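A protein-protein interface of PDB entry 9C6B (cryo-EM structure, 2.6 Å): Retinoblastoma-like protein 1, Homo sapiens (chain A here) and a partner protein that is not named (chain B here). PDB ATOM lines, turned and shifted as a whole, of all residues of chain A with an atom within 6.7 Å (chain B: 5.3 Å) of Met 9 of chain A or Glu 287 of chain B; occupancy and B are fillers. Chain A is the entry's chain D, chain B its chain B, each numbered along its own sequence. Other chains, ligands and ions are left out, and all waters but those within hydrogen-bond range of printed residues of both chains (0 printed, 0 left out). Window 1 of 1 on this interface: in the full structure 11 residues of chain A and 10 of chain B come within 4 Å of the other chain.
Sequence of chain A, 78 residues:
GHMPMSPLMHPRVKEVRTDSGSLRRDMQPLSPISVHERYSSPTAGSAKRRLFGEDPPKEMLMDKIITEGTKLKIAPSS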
ATOM      1  N   PRO A   7      23.718  27.580  14.395  1.00  0.00           N
ATOM      2  CA  PRO A   7      22.561  26.682  14.341  1.00  0.00           C
ATOM      3  C   PRO A   7      22.447  25.833  15.596  1.00  0.00           C
ATOM      4  O   PRO A   7      23.444  25.471  16.225  1.00  0.00           O
ATOM      5  CB  PRO A   7      22.844  25.816  13.109  1.00  0.00           C
ATOM      6  CG  PRO A   7      24.326  25.827  12.984  1.00  0.00           C
ATOM      7  CD  PRO A   7      24.768  27.189  13.439  1.00  0.00           C
ATOM      8  N   LEU A   8      21.207  25.516  15.955  1.00  0.00           N
ATOM      9  CA  LEU A   8      20.952  24.680  17.116  1.00  0.00           C
ATOM     10  C   LEU A   8      21.183  23.211  16.776  1.00  0.00           C
ATOM     11  O   LEU A   8      21.190  22.809  15.610  1.00  0.00           O
ATOM     12  CB  LEU A   8      19.529  24.884  17.638  1.00  0.00           C
ATOM     13  CG  LEU A   8      18.354  24.311  16.843  1.00  0.00           C
ATOM     14  CD1 LEU A   8      17.107  24.295  17.708  1.00  0.00           C
ATOM     15  CD2 LEU A   8      18.096  25.098  15.570  1.00  0.00           C
ATOM     16  N   MET A   9      21.375  22.409  17.816  1.00  0.00           N
ATOM     17  CA  MET A   9      21.722  21.009  17.645  1.00  0.00           C
ATOM     18  C   MET A   9      20.474  20.141  17.528  1.00  0.00           C
ATOM     19  O   MET A   9      19.358  20.559  17.841  1.00  0.00           O
ATOM     20  CB  MET A   9      22.587  20.519  18.807  1.00  0.00           C
ATOM     21  CG  MET A   9      21.884  20.529  20.154  1.00  0.00           C
ATOM     22  SD  MET A   9      22.976  20.041  21.503  1.00  0.00           S
ATOM     23  CE  MET A   9      24.008  21.496  21.645  1.00  0.00           C
ATOM     24  N   HIS A  10      20.685  18.915  17.062  1.00  0.00           N
ATOM     25  CA  HIS A  10      19.599  17.957  16.943  1.00  0.00           C
ATOM     26  C   HIS A  10      19.095  17.564  18.330  1.00  0.00           C
ATOM     27  O   HIS A  10      19.893  17.414  19.260  1.00  0.00           O
ATOM     28  CB  HIS A  10      20.074  16.721  16.181  1.00  0.00           C
ATOM     29  CG  HIS A  10      18.973  15.793  15.778  1.00  0.00           C
ATOM     30  ND1 HIS A  10      17.939  16.179  14.953  1.00  0.00           N
ATOM     31  CD2 HIS A  10      18.750  14.493  16.077  1.00  0.00           C
ATOM     32  CE1 HIS A  10      17.122  15.157  14.768  1.00  0.00           C
ATOM     33  NE2 HIS A  10      17.592  14.121  15.439  1.00  0.00           N
ATOM     34  N   PRO A  11      17.779  17.405  18.506  1.00  0.00           N
ATOM     35  CA  PRO A  11      17.262  17.042  19.836  1.00  0.00           C
ATOM     36  C   PRO A  11      17.808  15.733  20.374  1.00  0.00           C
ATOM     37  O   PRO A  11      18.024  15.616  21.586  1.00  0.00           O
ATOM     38  CB  PRO A  11      15.747  16.968  19.610  1.00  0.00           C
ATOM     39  CG  PRO A  11      15.501  17.843  18.446  1.00  0.00           C
ATOM     40  CD  PRO A  11      16.695  17.694  17.555  1.00  0.00           C
ATOM     41  N   ARG A  12      18.035  14.738  19.514  1.00  0.00           N
ATOM     42  CA  ARG A  12      18.534  13.456  19.998  1.00  0.00           C
ATOM     43  C   ARG A  12      19.909  13.606  20.630  1.00  0.00           C
ATOM     44  O   ARG A  12      20.208  12.958  21.641  1.00  0.00           O
ATOM     45  CB  ARG A  12      18.576  12.437  18.862  1.00  0.00           C
ATOM     46  CG  ARG A  12      17.236  11.802  18.558  1.00  0.00           C
ATOM     47  CD  ARG A  12      16.624  11.179  19.801  1.00  0.00           C
ATOM     48  NE  ARG A  12      17.488  10.172  20.401  1.00  0.00           N
ATOM     49  CZ  ARG A  12      17.334   9.690  21.627  1.00  0.00           C
ATOM     50  NH1 ARG A  12      16.364  10.116  22.419  1.00  0.00           N
ATOM     51  NH2 ARG A  12      18.172   8.758  22.069  1.00  0.00           N
ATOM     52  N   VAL A  13      20.757  14.459  20.054  1.00  0.00           N
ATOM     53  CA  VAL A  13      22.096  14.663  20.600  1.00  0.00           C
ATOM     54  C   VAL A  13      22.011  15.183  22.030  1.00  0.00           C
ATOM     55  O   VAL A  13      22.638  14.638  22.947  1.00  0.00           O
ATOM     56  CB  VAL A  13      22.899  15.620  19.704  1.00  0.00           C
ATOM     57  CG1 VAL A  13      24.331  15.719  20.187  1.00  0.00           C
ATOM     58  CG2 VAL A  13      22.849  15.159  18.260  1.00  0.00           C
ATOM     59  N   LYS A  14      21.219  16.235  22.242  1.00  0.00           N
ATOM     60  CA  LYS A  14      21.141  16.834  23.569  1.00  0.00           C
ATOM     61  C   LYS A  14      20.435  15.907  24.550  1.00  0.00           C
ATOM     62  O   LYS A  14      20.796  15.847  25.730  1.00  0.00           O
ATOM     63  CB  LYS A  14      20.460  18.207  23.493  1.00  0.00           C
ATOM     64  CG  LYS A  14      19.002  18.222  23.049  1.00  0.00           C
ATOM     65  CD  LYS A  14      18.039  18.102  24.223  1.00  0.00           C
ATOM     66  CE  LYS A  14      16.595  18.227  23.770  1.00  0.00           C
ATOM     67  NZ  LYS A  14      15.646  18.090  24.908  1.00  0.00           N
ATOM     68  N   GLU A  15      19.429  15.162  24.081  1.00  0.00           N
ATOM     69  CA  GLU A  15      18.758  14.211  24.962  1.00  0.00           C
ATOM     70  C   GLU A  15      19.719  13.128  25.430  1.00  0.00           C
ATOM     71  O   GLU A  15      19.773  12.807  26.622  1.00  0.00           O
ATOM     72  CB  GLU A  15      17.547  13.590  24.267  1.00  0.00           C
ATOM     73  CG  GLU A  15      16.416  14.561  23.994  1.00  0.00           C
ATOM     74  CD  GLU A  15      15.247  13.905  23.287  1.00  0.00           C
ATOM     75  OE1 GLU A  15      15.370  12.724  22.901  1.00  0.00           O
ATOM     76  OE2 GLU A  15      14.204  14.570  23.120  1.00  0.00           O
ATOM     77  N   ARG A  17      22.998  13.306  25.535  1.00  0.00           N
ATOM     78  CA  ARG A  17      24.013  13.931  26.377  1.00  0.00           C
ATOM     79  C   ARG A  17      23.499  14.151  27.795  1.00  0.00           C
ATOM     80  O   ARG A  17      24.160  13.778  28.772  1.00  0.00           O
ATOM     81  CB  ARG A  17      24.454  15.251  25.749  1.00  0.00           C
ATOM     82  CG  ARG A  17      25.603  15.928  26.458  1.00  0.00           C
ATOM     83  CD  ARG A  17      25.908  17.267  25.817  1.00  0.00           C
ATOM     84  NE  ARG A  17      26.354  17.118  24.439  1.00  0.00           N
ATOM     85  CZ  ARG A  17      26.535  18.127  23.599  1.00  0.00           C
ATOM     86  NH1 ARG A  17      26.310  19.378  23.963  1.00  0.00           N
ATOM     87  NH2 ARG A  17      26.952  17.874  22.362  1.00  0.00           N
ATOM     88  N   THR B 230      28.481  15.488  18.571  1.00  0.00           N
ATOM     89  CA  THR B 230      28.019  16.292  17.451  1.00  0.00           C
ATOM     90  C   THR B 230      27.070  15.562  16.516  1.00  0.00           C
ATOM     91  O   THR B 230      26.370  16.229  15.745  1.00  0.00           O
ATOM     92  CB  THR B 230      29.208  16.815  16.630  1.00  0.00           C
ATOM     93  OG1 THR B 230      30.048  15.718  16.252  1.00  0.00           O
ATOM     94  CG2 THR B 230      30.016  17.816  17.438  1.00  0.00           C
ATOM     95  N   SER B 251      23.097  12.323  12.041  1.00  0.00           N
ATOM     96  CA  SER B 251      22.275  13.520  12.152  1.00  0.00           C
ATOM     97  C   SER B 251      22.889  14.727  11.461  1.00  0.00           C
ATOM     98  O   SER B 251      22.216  15.755  11.347  1.00  0.00           O
ATOM     99  CB  SER B 251      22.021  13.843  13.623  1.00  0.00           C
ATOM    100  OG  SER B 251      23.235  13.894  14.345  1.00  0.00           O
ATOM    101  N   LYS B 252      24.137  14.640  11.012  1.00  0.00           N
ATOM    102  CA  LYS B 252      24.784  15.729  10.298  1.00  0.00           C
ATOM    103  C   LYS B 252      24.632  15.620   8.789  1.00  0.00           C
ATOM    104  O   LYS B 252      25.178  16.454   8.064  1.00  0.00           O
ATOM    105  CB  LYS B 252      26.268  15.794  10.666  1.00  0.00           C
ATOM    106  CG  LYS B 252      26.519  16.203  12.105  1.00  0.00           C
ATOM    107  CD  LYS B 252      28.001  16.248  12.423  1.00  0.00           C
ATOM    108  CE  LYS B 252      28.662  17.445  11.764  1.00  0.00           C
ATOM    109  NZ  LYS B 252      28.172  18.725  12.343  1.00  0.00           N
ATOM    110  N   PHE B 284      19.280  29.263  10.384  1.00  0.00           N
ATOM    111  CA  PHE B 284      19.360  28.796  11.762  1.00  0.00           C
ATOM    112  C   PHE B 284      19.091  27.299  11.859  1.00  0.00           C
ATOM    113  O   PHE B 284      19.755  26.608  12.637  1.00  0.00           O
ATOM    114  CB  PHE B 284      18.358  29.583  12.615  1.00  0.00           C
ATOM    115  CG  PHE B 284      18.329  29.196  14.072  1.00  0.00           C
ATOM    116  CD1 PHE B 284      19.439  28.653  14.698  1.00  0.00           C
ATOM    117  CD2 PHE B 284      17.175  29.375  14.816  1.00  0.00           C
ATOM    118  CE1 PHE B 284      19.400  28.305  16.032  1.00  0.00           C
ATOM    119  CE2 PHE B 284      17.129  29.025  16.150  1.00  0.00           C
ATOM    120  CZ  PHE B 284      18.242  28.489  16.759  1.00  0.00           C
ATOM    121  N   PHE B 285      18.158  26.779  11.065  1.00  0.00           N
ATOM    122  CA  PHE B 285      17.755  25.382  11.129  1.00  0.00           C
ATOM    123  C   PHE B 285      18.524  24.500  10.156  1.00  0.00           C
ATOM    124  O   PHE B 285      18.126  23.354   9.932  1.00  0.00           O
ATOM    125  CB  PHE B 285      16.255  25.254  10.860  1.00  0.00           C
ATOM    126  CG  PHE B 285      15.416  26.234  11.623  1.00  0.00           C
ATOM    127  CD1 PHE B 285      14.967  25.936  12.896  1.00  0.00           C
ATOM    128  CD2 PHE B 285      15.066  27.449  11.062  1.00  0.00           C
ATOM    129  CE1 PHE B 285      14.193  26.835  13.598  1.00  0.00           C
ATOM    130  CE2 PHE B 285      14.293  28.350  11.760  1.00  0.00           C
ATOM    131  CZ  PHE B 285      13.856  28.043  13.028  1.00  0.00           C
ATOM    132  N   SER B 286      19.615  25.005   9.576  1.00  0.00           N
ATOM    133  CA  SER B 286      20.333  24.251   8.554  1.00  0.00           C
ATOM    134  C   SER B 286      20.918  22.952   9.088  1.00  0.00           C
ATOM    135  O   SER B 286      21.258  22.069   8.293  1.00  0.00           O
ATOM    136  CB  SER B 286      21.445  25.110   7.952  1.00  0.00           C
ATOM    137  OG  SER B 286      22.268  25.657   8.965  1.00  0.00           O
ATOM    138  N   GLU B 287      21.047  22.810  10.404  1.00  0.00           N
ATOM    139  CA  GLU B 287      21.542  21.567  10.976  1.00  0.00           C
ATOM    140  C   GLU B 287      20.421  20.573  11.245  1.00  0.00           C
ATOM    141  O   GLU B 287      20.656  19.360  11.208  1.00  0.00           O
ATOM    142  CB  GLU B 287      22.317  21.856  12.266  1.00  0.00           C
ATOM    143  CG  GLU B 287      23.089  20.672  12.845  1.00  0.00           C
ATOM    144  CD  GLU B 287      22.235  19.756  13.700  1.00  0.00           C
ATOM    145  OE1 GLU B 287      21.255  20.243  14.300  1.00  0.00           O
ATOM    146  OE2 GLU B 287      22.544  18.549  13.772  1.00  0.00           O
ATOM    147  N   ILE B 288      19.206  21.058  11.500  1.00  0.00           N
ATOM    148  CA  ILE B 288      18.087  20.157  11.750  1.00  0.00           C
ATOM    149  C   ILE B 288      17.550  19.582  10.447  1.00  0.00           C
ATOM    150  O   ILE B 288      17.356  18.368  10.324  1.00  0.00           O
ATOM    151  CB  ILE B 288      16.984  20.883  12.537  1.00  0.00           C
ATOM    152  CG1 ILE B 288      17.461  21.210  13.949  1.00  0.00           C
ATOM    153  CG2 ILE B 288      15.725  20.042  12.586  1.00  0.00           C
ATOM    154  CD1 ILE B 288      16.439  21.958  14.766  1.00  0.00           C
ATOM    155  N   ILE B 289      17.303  20.438   9.452  1.00  0.00           N
ATOM    156  CA  ILE B 289      16.725  19.977   8.192  1.00  0.00           C
ATOM    157  C   ILE B 289      17.694  19.160   7.355  1.00  0.00           C
ATOM    158  O   ILE B 289      17.280  18.574   6.348  1.00  0.00           O
ATOM    159  CB  ILE B 289      16.212  21.165   7.358  1.00  0.00           C
ATOM    160  CG1 ILE B 289      17.382  21.936   6.752  1.00  0.00           C
ATOM    161  CG2 ILE B 289      15.360  22.081   8.212  1.00  0.00           C
ATOM    162  CD1 ILE B 289      16.961  23.145   5.954  1.00  0.00           C
ATOM    163  N   SER B 290      18.971  19.111   7.731  1.00  0.00           N
ATOM    164  CA  SER B 290      19.952  18.298   7.026  1.00  0.00           C
ATOM    165  C   SER B 290      20.111  16.905   7.618  1.00  0.00           C
ATOM    166  O   SER B 290      20.796  16.072   7.019  1.00  0.00           O
ATOM    167  CB  SER B 290      21.314  19.000   7.014  1.00  0.00           C
ATOM    168  OG  SER B 290      21.857  19.072   8.320  1.00  0.00           O
ATOM    169  N   SER B 291      19.506  16.635   8.769  1.00  0.00           N
ATOM    170  CA  SER B 291      19.574  15.306   9.356  1.00  0.00           C
ATOM    171  C   SER B 291      18.808  14.310   8.498  1.00  0.00           C
ATOM    172  O   SER B 291      17.717  14.602   8.004  1.00  0.00           O
ATOM    173  CB  SER B 291      19.008  15.321  10.772  1.00  0.00           C
ATOM    174  OG  SER B 291      18.745  14.006  11.224  1.00  0.00           O
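The side-chain carboxylate (OE1) of Glu 287 of chain B sits close to the backbone carbonyl oxygen (O) of Leu 8 of chain A, 2.9 Å away.
The side-chain carboxylate of Glu 287 of chain B lies within hydrogen-bond range of the backbone NH of His 10 of chain A (3.1 Å).
The side-chain hydroxyl (OG) of Ser 290 of chain B sits at hydrogen-bond distance from the backbone carbonyl oxygen (O) of Glu 287 of chain B (3.1 Å).
Pro 7 of chain A touches Phe 284 of chain B (CB to O, 3.2 Å).
Leu 8 of chain A touches Phe 284 of chain B (N to CE1, 3.3 Å).
Leu 8 of chain A touches Ile 288 of chain B.
Met 9 of chain A touches Glu 287 of chain B (C to OE1, 3.3 Å).
Met 9 of chain A touches just one residue of chain B: Glu 287 (3.3 Å).
Of chain A, only Leu 8 (2.9 Å), Met 9 (3.3 Å) and His 10 (3.1 Å) come within 4 Å of Glu 287 of chain B.
Of the printed residues of chain B, His 10 of chain A touches Glu 287 (3.1 Å).
Printed residues of chain B within 4 Å of Leu 8 of chain A: Phe 284, Glu 287 and Ile 288.
Ile 289 of chain B touches none of the printed residues of chain A.
The nearest residue of chain B that does not touch Met 9 of chain A is Ile 288 of chain B (4.4 Å).
The nearest printed residue of chain B that does not touch Pro 7 of chain A is Glu 287 of chain B (4.1 Å).
Hydrophobic or aromatic side chains of chain A within 4 Å of the printed part of chain B: Pro 7, Leu 8 and His 10.
Along chain B the printed residues that touch a printed residue of chain A span positions 284 to 288.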
